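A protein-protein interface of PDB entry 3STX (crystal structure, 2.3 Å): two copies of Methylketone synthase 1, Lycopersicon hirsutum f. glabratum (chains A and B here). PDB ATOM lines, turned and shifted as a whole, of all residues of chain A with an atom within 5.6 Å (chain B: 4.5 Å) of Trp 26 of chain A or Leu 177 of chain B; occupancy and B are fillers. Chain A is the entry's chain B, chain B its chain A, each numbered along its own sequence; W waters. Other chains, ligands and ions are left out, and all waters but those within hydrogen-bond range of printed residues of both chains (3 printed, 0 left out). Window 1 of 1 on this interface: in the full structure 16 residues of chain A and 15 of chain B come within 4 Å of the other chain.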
ATOM      1  N   PHE A  22      -1.438  -3.628  -9.598  1.00  0.00           N
ATOM      2  CA  PHE A  22      -2.535  -2.711  -9.223  1.00  0.00           C
ATOM      3  C   PHE A  22      -2.325  -2.062  -7.853  1.00  0.00           C
ATOM      4  O   PHE A  22      -2.947  -1.043  -7.536  1.00  0.00           O
ATOM      5  CB  PHE A  22      -3.907  -3.404  -9.239  1.00  0.00           C
ATOM      6  CG  PHE A  22      -4.157  -4.279 -10.446  1.00  0.00           C
ATOM      7  CD1 PHE A  22      -4.207  -3.738 -11.719  1.00  0.00           C
ATOM      8  CD2 PHE A  22      -4.395  -5.646 -10.288  1.00  0.00           C
ATOM      9  CE1 PHE A  22      -4.464  -4.539 -12.829  1.00  0.00           C
ATOM     10  CE2 PHE A  22      -4.646  -6.467 -11.392  1.00  0.00           C
ATOM     11  CZ  PHE A  22      -4.682  -5.904 -12.668  1.00  0.00           C
ATOM     12  N   HIS A  23      -1.463  -2.664  -7.043  1.00  0.00           N
ATOM     13  CA  HIS A  23      -1.322  -2.256  -5.655  1.00  0.00           C
ATOM     14  C   HIS A  23      -0.138  -1.322  -5.453  1.00  0.00           C
ATOM     15  O   HIS A  23       0.314  -0.680  -6.394  1.00  0.00           O
ATOM     16  CB  HIS A  23      -1.276  -3.485  -4.745  1.00  0.00           C
ATOM     17  CG  HIS A  23      -2.583  -4.212  -4.662  1.00  0.00           C
ATOM     18  ND1 HIS A  23      -3.145  -4.862  -5.743  1.00  0.00           N
ATOM     19  CD2 HIS A  23      -3.447  -4.379  -3.633  1.00  0.00           C
ATOM     20  CE1 HIS A  23      -4.294  -5.402  -5.382  1.00  0.00           C
ATOM     21  NE2 HIS A  23      -4.501  -5.127  -4.106  1.00  0.00           N
ATOM     22  N   GLY A  24       0.355  -1.239  -4.224  1.00  0.00           N
ATOM     23  CA  GLY A  24       1.369  -0.253  -3.854  1.00  0.00           C
ATOM     24  C   GLY A  24       1.667  -0.437  -2.388  1.00  0.00           C
ATOM     25  O   GLY A  24       0.983  -1.212  -1.718  1.00  0.00           O
ATOM     26  N   ALA A  25       2.690   0.256  -1.890  1.00  0.00           N
ATOM     27  CA  ALA A  25       3.153   0.090  -0.502  1.00  0.00           C
ATOM     28  C   ALA A  25       2.024   0.105   0.529  1.00  0.00           C
ATOM     29  O   ALA A  25       2.116  -0.571   1.561  1.00  0.00           O
ATOM     30  CB  ALA A  25       4.191   1.148  -0.158  1.00  0.00           C
ATOM     31  N   TRP A  26       0.978   0.886   0.245  1.00  0.00           N
ATOM     32  CA  TRP A  26      -0.230   0.970   1.078  1.00  0.00           C
ATOM     33  C   TRP A  26      -0.885  -0.375   1.461  1.00  0.00           C
ATOM     34  O   TRP A  26      -1.463  -0.491   2.549  1.00  0.00           O
ATOM     35  CB  TRP A  26      -1.279   1.861   0.398  1.00  0.00           C
ATOM     36  CG  TRP A  26      -1.696   1.367  -0.943  1.00  0.00           C
ATOM     37  CD1 TRP A  26      -1.134   1.688  -2.138  1.00  0.00           C
ATOM     38  CD2 TRP A  26      -2.775   0.462  -1.235  1.00  0.00           C
ATOM     39  NE1 TRP A  26      -1.786   1.042  -3.157  1.00  0.00           N
ATOM     40  CE2 TRP A  26      -2.796   0.282  -2.635  1.00  0.00           C
ATOM     41  CE3 TRP A  26      -3.717  -0.216  -0.451  1.00  0.00           C
ATOM     42  CZ2 TRP A  26      -3.722  -0.553  -3.272  1.00  0.00           C
ATOM     43  CZ3 TRP A  26      -4.634  -1.047  -1.078  1.00  0.00           C
ATOM     44  CH2 TRP A  26      -4.635  -1.204  -2.479  1.00  0.00           C
ATOM     45  N   CYS A  27      -0.808  -1.381   0.585  1.00  0.00           N
ATOM     46  CA  CYS A  27      -1.502  -2.659   0.850  1.00  0.00           C
ATOM     47  C   CYS A  27      -0.947  -3.371   2.092  1.00  0.00           C
ATOM     48  O   CYS A  27      -1.646  -4.157   2.744  1.00  0.00           O
ATOM     49  CB  CYS A  27      -1.478  -3.581  -0.381  1.00  0.00           C
ATOM     50  SG  CYS A  27       0.125  -4.363  -0.722  1.00  0.00           S
ATOM     51  N   TRP A  28       0.308  -3.062   2.412  1.00  0.00           N
ATOM     52  CA  TRP A  28       1.030  -3.638   3.538  1.00  0.00           C
ATOM     53  C   TRP A  28       0.819  -2.906   4.871  1.00  0.00           C
ATOM     54  O   TRP A  28       1.491  -3.221   5.851  1.00  0.00           O
ATOM     55  CB  TRP A  28       2.531  -3.639   3.227  1.00  0.00           C
ATOM     56  CG  TRP A  28       2.953  -4.459   2.034  1.00  0.00           C
ATOM     57  CD1 TRP A  28       3.191  -4.002   0.774  1.00  0.00           C
ATOM     58  CD2 TRP A  28       3.223  -5.866   2.009  1.00  0.00           C
ATOM     59  NE1 TRP A  28       3.587  -5.032  -0.040  1.00  0.00           N
ATOM     60  CE2 TRP A  28       3.617  -6.190   0.690  1.00  0.00           C
ATOM     61  CE3 TRP A  28       3.177  -6.886   2.975  1.00  0.00           C
ATOM     62  CZ2 TRP A  28       3.954  -7.499   0.303  1.00  0.00           C
ATOM     63  CZ3 TRP A  28       3.515  -8.193   2.589  1.00  0.00           C
ATOM     64  CH2 TRP A  28       3.901  -8.481   1.265  1.00  0.00           C
ATOM     65  N   TYR A  29      -0.113  -1.950   4.923  1.00  0.00           N
ATOM     66  CA  TYR A  29      -0.292  -1.105   6.122  1.00  0.00           C
ATOM     67  C   TYR A  29      -0.369  -1.822   7.483  1.00  0.00           C
ATOM     68  O   TYR A  29       0.247  -1.369   8.465  1.00  0.00           O
ATOM     69  CB  TYR A  29      -1.412  -0.084   5.939  1.00  0.00           C
ATOM     70  CG  TYR A  29      -2.826  -0.592   6.093  1.00  0.00           C
ATOM     71  CD1 TYR A  29      -3.553  -0.312   7.243  1.00  0.00           C
ATOM     72  CD2 TYR A  29      -3.449  -1.325   5.078  1.00  0.00           C
ATOM     73  CE1 TYR A  29      -4.849  -0.763   7.398  1.00  0.00           C
ATOM     74  CE2 TYR A  29      -4.758  -1.785   5.227  1.00  0.00           C
ATOM     75  CZ  TYR A  29      -5.448  -1.486   6.387  1.00  0.00           C
ATOM     76  OH  TYR A  29      -6.730  -1.906   6.559  1.00  0.00           O
ATOM     77  N   LYS A  30      -1.101  -2.936   7.540  1.00  0.00           N
ATOM     78  CA  LYS A  30      -1.201  -3.724   8.777  1.00  0.00           C
ATOM     79  C   LYS A  30       0.120  -4.399   9.148  1.00  0.00           C
ATOM     80  O   LYS A  30       0.487  -4.452  10.319  1.00  0.00           O
ATOM     81  CB  LYS A  30      -2.294  -4.780   8.667  1.00  0.00           C
ATOM     82  CG  LYS A  30      -3.672  -4.229   8.389  1.00  0.00           C
ATOM     83  CD  LYS A  30      -4.516  -5.303   7.732  1.00  0.00           C
ATOM     84  CE  LYS A  30      -5.955  -4.867   7.603  1.00  0.00           C
ATOM     85  NZ  LYS A  30      -6.774  -5.990   7.123  1.00  0.00           N
ATOM     86  N   ASP A  46       6.511   1.499  -3.321  1.00  0.00           N
ATOM     87  CA  ASP A  46       5.755   1.609  -4.557  1.00  0.00           C
ATOM     88  C   ASP A  46       6.714   1.334  -5.703  1.00  0.00           C
ATOM     89  O   ASP A  46       7.768   1.951  -5.785  1.00  0.00           O
ATOM     90  CB  ASP A  46       5.183   3.018  -4.740  1.00  0.00           C
ATOM     91  CG  ASP A  46       4.247   3.433  -3.629  1.00  0.00           C
ATOM     92  OD1 ASP A  46       3.355   2.641  -3.246  1.00  0.00           O
ATOM     93  OD2 ASP A  46       4.385   4.585  -3.159  1.00  0.00           O
ATOM     94  N   GLY A  51       0.721   2.865  -6.272  1.00  0.00           N
ATOM     95  CA  GLY A  51       0.483   3.754  -5.135  1.00  0.00           C
ATOM     96  C   GLY A  51       0.692   5.212  -5.487  1.00  0.00           C
ATOM     97  O   GLY A  51       0.083   5.723  -6.432  1.00  0.00           O
ATOM     98  N   TYR A 167     -10.117 -10.032  -2.794  1.00  0.00           N
ATOM     99  CA  TYR A 167     -10.443  -9.600  -1.437  1.00  0.00           C
ATOM    100  C   TYR A 167     -11.514 -10.424  -0.736  1.00  0.00           C
ATOM    101  O   TYR A 167     -11.986 -10.043   0.344  1.00  0.00           O
ATOM    102  CB  TYR A 167     -10.837  -8.122  -1.451  1.00  0.00           C
ATOM    103  CG  TYR A 167      -9.636  -7.221  -1.471  1.00  0.00           C
ATOM    104  CD1 TYR A 167      -8.932  -7.000  -2.653  1.00  0.00           C
ATOM    105  CD2 TYR A 167      -9.186  -6.604  -0.302  1.00  0.00           C
ATOM    106  CE1 TYR A 167      -7.814  -6.193  -2.673  1.00  0.00           C
ATOM    107  CE2 TYR A 167      -8.075  -5.785  -0.316  1.00  0.00           C
ATOM    108  CZ  TYR A 167      -7.390  -5.593  -1.504  1.00  0.00           C
ATOM    109  OH  TYR A 167      -6.289  -4.785  -1.534  1.00  0.00           O
ATOM    110  N   ASP A 174     -11.260  -3.005   3.717  1.00  0.00           N
ATOM    111  CA  ASP A 174     -10.079  -3.242   2.884  1.00  0.00           C
ATOM    112  C   ASP A 174     -10.398  -3.321   1.402  1.00  0.00           C
ATOM    113  O   ASP A 174      -9.593  -2.900   0.571  1.00  0.00           O
ATOM    114  CB  ASP A 174      -9.368  -4.519   3.325  1.00  0.00           C
ATOM    115  CG  ASP A 174      -8.884  -4.441   4.750  1.00  0.00           C
ATOM    116  OD1 ASP A 174      -8.619  -3.318   5.240  1.00  0.00           O
ATOM    117  OD2 ASP A 174      -8.779  -5.506   5.386  1.00  0.00           O
ATOM    118  N   LEU A 177     -10.851   0.328   0.571  1.00  0.00           N
ATOM    119  CA  LEU A 177      -9.517   0.926   0.474  1.00  0.00           C
ATOM    120  C   LEU A 177      -8.921   0.694  -0.913  1.00  0.00           C
ATOM    121  O   LEU A 177      -8.421   1.621  -1.563  1.00  0.00           O
ATOM    122  CB  LEU A 177      -8.601   0.354   1.558  1.00  0.00           C
ATOM    123  CG  LEU A 177      -7.235   1.028   1.759  1.00  0.00           C
ATOM    124  CD1 LEU A 177      -7.378   2.507   2.154  1.00  0.00           C
ATOM    125  CD2 LEU A 177      -6.417   0.269   2.786  1.00  0.00           C
ATOM    126  N   ALA A 178      -9.019  -0.552  -1.365  1.00  0.00           N
ATOM    127  CA  ALA A 178      -8.490  -0.979  -2.656  1.00  0.00           C
ATOM    128  C   ALA A 178      -9.207  -0.364  -3.854  1.00  0.00           C
ATOM    129  O   ALA A 178      -8.548   0.109  -4.782  1.00  0.00           O
ATOM    130  CB  ALA A 178      -8.490  -2.489  -2.741  1.00  0.00           C
ATOM    131  N   LEU A 181      -7.725   2.843  -4.486  1.00  0.00           N
ATOM    132  CA  LEU A 181      -6.250   2.958  -4.671  1.00  0.00           C
ATOM    133  C   LEU A 181      -5.606   2.148  -5.802  1.00  0.00           C
ATOM    134  O   LEU A 181      -4.500   2.472  -6.244  1.00  0.00           O
ATOM    135  CB  LEU A 181      -5.507   2.663  -3.365  1.00  0.00           C
ATOM    136  CG  LEU A 181      -5.631   3.720  -2.267  1.00  0.00           C
ATOM    137  CD1 LEU A 181      -5.352   3.108  -0.904  1.00  0.00           C
ATOM    138  CD2 LEU A 181      -4.745   4.943  -2.531  1.00  0.00           C
ATOM    139  N   VAL A 182      -6.272   1.090  -6.257  1.00  0.00           N
ATOM    140  CA  VAL A 182      -5.734   0.278  -7.356  1.00  0.00           C
ATOM    141  C   VAL A 182      -5.465   1.127  -8.599  1.00  0.00           C
ATOM    142  O   VAL A 182      -6.227   2.049  -8.929  1.00  0.00           O
ATOM    143  CB  VAL A 182      -6.635  -0.941  -7.722  1.00  0.00           C
ATOM    144  CG1 VAL A 182      -6.674  -1.946  -6.578  1.00  0.00           C
ATOM    145  CG2 VAL A 182      -8.037  -0.494  -8.092  1.00  0.00           C
ATOM    146  N   MET A 249      -3.981  -8.538   3.950  1.00  0.00           N
ATOM    147  CA  MET A 249      -5.280  -8.001   4.356  1.00  0.00           C
ATOM    148  C   MET A 249      -6.111  -9.000   5.151  1.00  0.00           C
ATOM    149  O   MET A 249      -6.769  -8.619   6.125  1.00  0.00           O
ATOM    150  CB  MET A 249      -6.107  -7.557   3.142  1.00  0.00           C
ATOM    151  CG  MET A 249      -5.448  -6.549   2.254  1.00  0.00           C
ATOM    152  SD  MET A 249      -5.339  -4.919   2.982  1.00  0.00           S
ATOM    153  CE  MET A 249      -4.866  -3.987   1.537  1.00  0.00           C
ATOM    154  N   TRP B  26      -8.906   7.672  -0.230  1.00  0.00           N
ATOM    155  CA  TRP B  26      -8.468   6.557   0.629  1.00  0.00           C
ATOM    156  C   TRP B  26      -8.745   6.733   2.124  1.00  0.00           C
ATOM    157  O   TRP B  26      -9.131   5.783   2.811  1.00  0.00           O
ATOM    158  CB  TRP B  26      -6.979   6.237   0.397  1.00  0.00           C
ATOM    159  CG  TRP B  26      -6.053   7.368   0.704  1.00  0.00           C
ATOM    160  CD1 TRP B  26      -5.564   8.295  -0.181  1.00  0.00           C
ATOM    161  CD2 TRP B  26      -5.511   7.713   1.984  1.00  0.00           C
ATOM    162  NE1 TRP B  26      -4.753   9.187   0.473  1.00  0.00           N
ATOM    163  CE2 TRP B  26      -4.705   8.853   1.802  1.00  0.00           C
ATOM    164  CE3 TRP B  26      -5.621   7.162   3.268  1.00  0.00           C
ATOM    165  CZ2 TRP B  26      -4.014   9.457   2.856  1.00  0.00           C
ATOM    166  CZ3 TRP B  26      -4.938   7.767   4.312  1.00  0.00           C
ATOM    167  CH2 TRP B  26      -4.143   8.899   4.097  1.00  0.00           C
ATOM    168  N   TYR B  29     -11.970   5.243   3.752  1.00  0.00           N
ATOM    169  CA  TYR B  29     -12.290   3.824   3.489  1.00  0.00           C
ATOM    170  C   TYR B  29     -13.229   3.172   4.508  1.00  0.00           C
ATOM    171  O   TYR B  29     -14.134   2.421   4.134  1.00  0.00           O
ATOM    172  CB  TYR B  29     -11.021   2.981   3.273  1.00  0.00           C
ATOM    173  CG  TYR B  29     -10.255   2.594   4.520  1.00  0.00           C
ATOM    174  CD1 TYR B  29     -10.190   1.260   4.931  1.00  0.00           C
ATOM    175  CD2 TYR B  29      -9.568   3.548   5.273  1.00  0.00           C
ATOM    176  CE1 TYR B  29      -9.473   0.888   6.067  1.00  0.00           C
ATOM    177  CE2 TYR B  29      -8.861   3.187   6.416  1.00  0.00           C
ATOM    178  CZ  TYR B  29      -8.817   1.855   6.805  1.00  0.00           C
ATOM    179  OH  TYR B  29      -8.109   1.488   7.929  1.00  0.00           O
ATOM    180  N   GLU B 173      -2.113   1.275  12.561  1.00  0.00           N
ATOM    181  CA  GLU B 173      -2.100   0.817  11.177  1.00  0.00           C
ATOM    182  C   GLU B 173      -2.498   1.947  10.224  1.00  0.00           C
ATOM    183  O   GLU B 173      -1.914   2.089   9.149  1.00  0.00           O
ATOM    184  CB  GLU B 173      -2.927  -0.473  10.977  1.00  0.00           C
ATOM    185  CG  GLU B 173      -4.423  -0.428  11.350  1.00  0.00           C
ATOM    186  CD  GLU B 173      -4.706  -0.807  12.801  1.00  0.00           C
ATOM    187  OE1 GLU B 173      -5.822  -1.316  13.084  1.00  0.00           O
ATOM    188  OE2 GLU B 173      -3.830  -0.591  13.668  1.00  0.00           O
ATOM    189  N   ASP B 174      -3.462   2.767  10.648  1.00  0.00           N
ATOM    190  CA  ASP B 174      -3.911   3.946   9.882  1.00  0.00           C
ATOM    191  C   ASP B 174      -2.843   5.050   9.767  1.00  0.00           C
ATOM    192  O   ASP B 174      -2.772   5.759   8.752  1.00  0.00           O
ATOM    193  CB  ASP B 174      -5.208   4.506  10.475  1.00  0.00           C
ATOM    194  CG  ASP B 174      -6.401   3.582  10.244  1.00  0.00           C
ATOM    195  OD1 ASP B 174      -6.670   3.194   9.084  1.00  0.00           O
ATOM    196  OD2 ASP B 174      -7.064   3.228  11.225  1.00  0.00           O
ATOM    197  N   LEU B 175      -2.028   5.201  10.811  1.00  0.00           N
ATOM    198  CA  LEU B 175      -0.841   6.051  10.726  1.00  0.00           C
ATOM    199  C   LEU B 175       0.046   5.512   9.603  1.00  0.00           C
ATOM    200  O   LEU B 175       0.373   6.241   8.666  1.00  0.00           O
ATOM    201  CB  LEU B 175      -0.084   6.095  12.061  1.00  0.00           C
ATOM    202  CG  LEU B 175       1.332   6.699  11.999  1.00  0.00           C
ATOM    203  CD1 LEU B 175       1.276   8.196  11.706  1.00  0.00           C
ATOM    204  CD2 LEU B 175       2.146   6.396  13.279  1.00  0.00           C
ATOM    205  N   ALA B 176       0.387   4.224   9.691  1.00  0.00           N
ATOM    206  CA  ALA B 176       1.142   3.530   8.647  1.00  0.00           C
ATOM    207  C   ALA B 176       0.506   3.723   7.271  1.00  0.00           C
ATOM    208  O   ALA B 176       1.201   4.073   6.322  1.00  0.00           O
ATOM    209  CB  ALA B 176       1.273   2.058   8.971  1.00  0.00           C
ATOM    210  N   LEU B 177      -0.810   3.507   7.174  1.00  0.00           N
ATOM    211  CA  LEU B 177      -1.549   3.752   5.926  1.00  0.00           C
ATOM    212  C   LEU B 177      -1.320   5.156   5.371  1.00  0.00           C
ATOM    213  O   LEU B 177      -0.964   5.318   4.207  1.00  0.00           O
ATOM    214  CB  LEU B 177      -3.057   3.510   6.105  1.00  0.00           C
ATOM    215  CG  LEU B 177      -3.901   3.594   4.825  1.00  0.00           C
ATOM    216  CD1 LEU B 177      -3.393   2.617   3.778  1.00  0.00           C
ATOM    217  CD2 LEU B 177      -5.386   3.356   5.120  1.00  0.00           C
ATOM    218  N   ALA B 178      -1.540   6.162   6.212  1.00  0.00           N
ATOM    219  CA  ALA B 178      -1.320   7.558   5.841  1.00  0.00           C
ATOM    220  C   ALA B 178       0.120   7.811   5.381  1.00  0.00           C
ATOM    221  O   ALA B 178       0.347   8.420   4.338  1.00  0.00           O
ATOM    222  CB  ALA B 178      -1.674   8.458   6.992  1.00  0.00           C
ATOM    223  N   THR B 179       1.079   7.311   6.151  1.00  0.00           N
ATOM    224  CA  THR B 179       2.520   7.483   5.881  1.00  0.00           C
ATOM    225  C   THR B 179       2.912   7.041   4.460  1.00  0.00           C
ATOM    226  O   THR B 179       3.732   7.689   3.796  1.00  0.00           O
ATOM    227  CB  THR B 179       3.327   6.752   6.979  1.00  0.00           C
ATOM    228  OG1 THR B 179       2.996   7.336   8.246  1.00  0.00           O
ATOM    229  CG2 THR B 179       4.856   6.824   6.754  1.00  0.00           C
ATOM    230  N   ALA B 180       2.285   5.970   3.983  1.00  0.00           N
ATOM    231  CA  ALA B 180       2.496   5.482   2.620  1.00  0.00           C
ATOM    232  C   ALA B 180       1.608   6.169   1.550  1.00  0.00           C
ATOM    233  O   ALA B 180       1.616   5.765   0.380  1.00  0.00           O
ATOM    234  CB  ALA B 180       2.305   3.956   2.576  1.00  0.00           C
ATOM    235  N   LEU B 181       0.841   7.192   1.928  1.00  0.00           N
ATOM    236  CA  LEU B 181      -0.142   7.734   0.985  1.00  0.00           C
ATOM    237  C   LEU B 181      -0.232   9.255   0.876  1.00  0.00           C
ATOM    238  O   LEU B 181      -0.694   9.771  -0.146  1.00  0.00           O
ATOM    239  CB  LEU B 181      -1.538   7.145   1.254  1.00  0.00           C
ATOM    240  CG  LEU B 181      -1.793   5.685   0.864  1.00  0.00           C
ATOM    241  CD1 LEU B 181      -3.186   5.260   1.309  1.00  0.00           C
ATOM    242  CD2 LEU B 181      -1.610   5.469  -0.629  1.00  0.00           C
HETATM  243  O   HOH W   1       3.925   5.238  -0.272  1.00  0.00           O
HETATM  244  O   HOH W   2      -8.683  -0.814   9.065  1.00  0.00           O
HETATM  245  O   HOH W   3       1.557   3.702  -1.596  1.00  0.00           O
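OH of Tyr 29 of chain B sits at hydrogen-bond distance from OD1 of Asp 174 of chain B (2.5 Å).
OH of Tyr 29 of chain A lies within hydrogen-bond range of OD1 of Asp 174 of chain A (2.7 Å).
Water W1 lies within hydrogen-bond range of O of Ala 180 of chain B and OD2 of Asp 46 of chain A.
Water W2 lies within hydrogen-bond range of OH of Tyr 29 of chain B (2.6 Å) and OH of Tyr 29 of chain A (3.4 Å).
Water W3 lies within hydrogen-bond range of the side-chain carboxylate of Asp 46 of chain A, the backbone carbonyl oxygen of Ala 180 of chain B and the backbone NH of Trp 26 of chain A.
Among the printed residues, merely in contact across the chains: Tyr 29 of chain A with Glu 173 of chain B (3.5 Å), Tyr 29 of chain A with Ala 176 of chain B (3.6 Å), Leu 177 of chain A with Leu 177 of chain B (3.7 Å), Leu 181 of chain A with Leu 181 of chain B (3.7 Å), Leu 177 of chain A with Tyr 29 of chain B (3.7 Å), Leu 181 of chain A with Trp 26 of chain B (3.8 Å), Trp 26 of chain A with Leu 181 of chain B (3.8 Å), Leu 177 of chain A with Trp 26 of chain B (3.8 Å), Tyr 29 of chain A with Leu 177 of chain B (3.8 Å), Trp 26 of chain A with Leu 177 of chain B (3.9 Å) and Tyr 29 of chain A with Tyr 29 of chain B (3.9 Å).
Printed residues of chain B that touch a printed residue of chain A: Trp 26, Tyr 29, Glu 173, Ala 176, Leu 177 and Leu 181.
Hydrophobic or aromatic side chains of chain A within 4 Å of the printed part of chain B: Trp 26, Tyr 29, Leu 177 and Leu 181.
Among the printed residues, no Asp or Glu carboxylate lies within 4 Å of a Lys or Arg side-chain nitrogen of the other chain.
Trp 26 of chain A touches Leu 177 of chain B, and with the chains exchanged Leu 177 of chain A touches Trp 26 of chain B.
Trp 26 of chain A touches Leu 181 of chain B, and with the chains exchanged Leu 181 of chain A touches Trp 26 of chain B.
Tyr 29 of chain A touches its own counterpart, Tyr 29 of chain B.
Leu 181 of chain B touches its own counterpart, Leu 181 of chain A.
Positions printed for both chains: 26, 29, 174, 177, 178 and 181.
His 23 of chain A touches none of the printed residues of chain B.
Of chain B, only Leu 177 and Leu 181 come within 4 Å of Trp 26 of chain A.
Asp 46 of chain A touches none of the printed residues of chain B.
Of the printed residues of chain B, Leu 177 of chain A touches Trp 26, Tyr 29 and Leu 177.
Of chain A, only Trp 26 (3.9 Å), Tyr 29 (3.8 Å) and Leu 177 (3.7 Å) come within 4 Å of Leu 177 of chain B.
Of the printed residues of chain A, Leu 181 of chain B touches Trp 26 (3.8 Å) and Leu 181 (3.7 Å).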
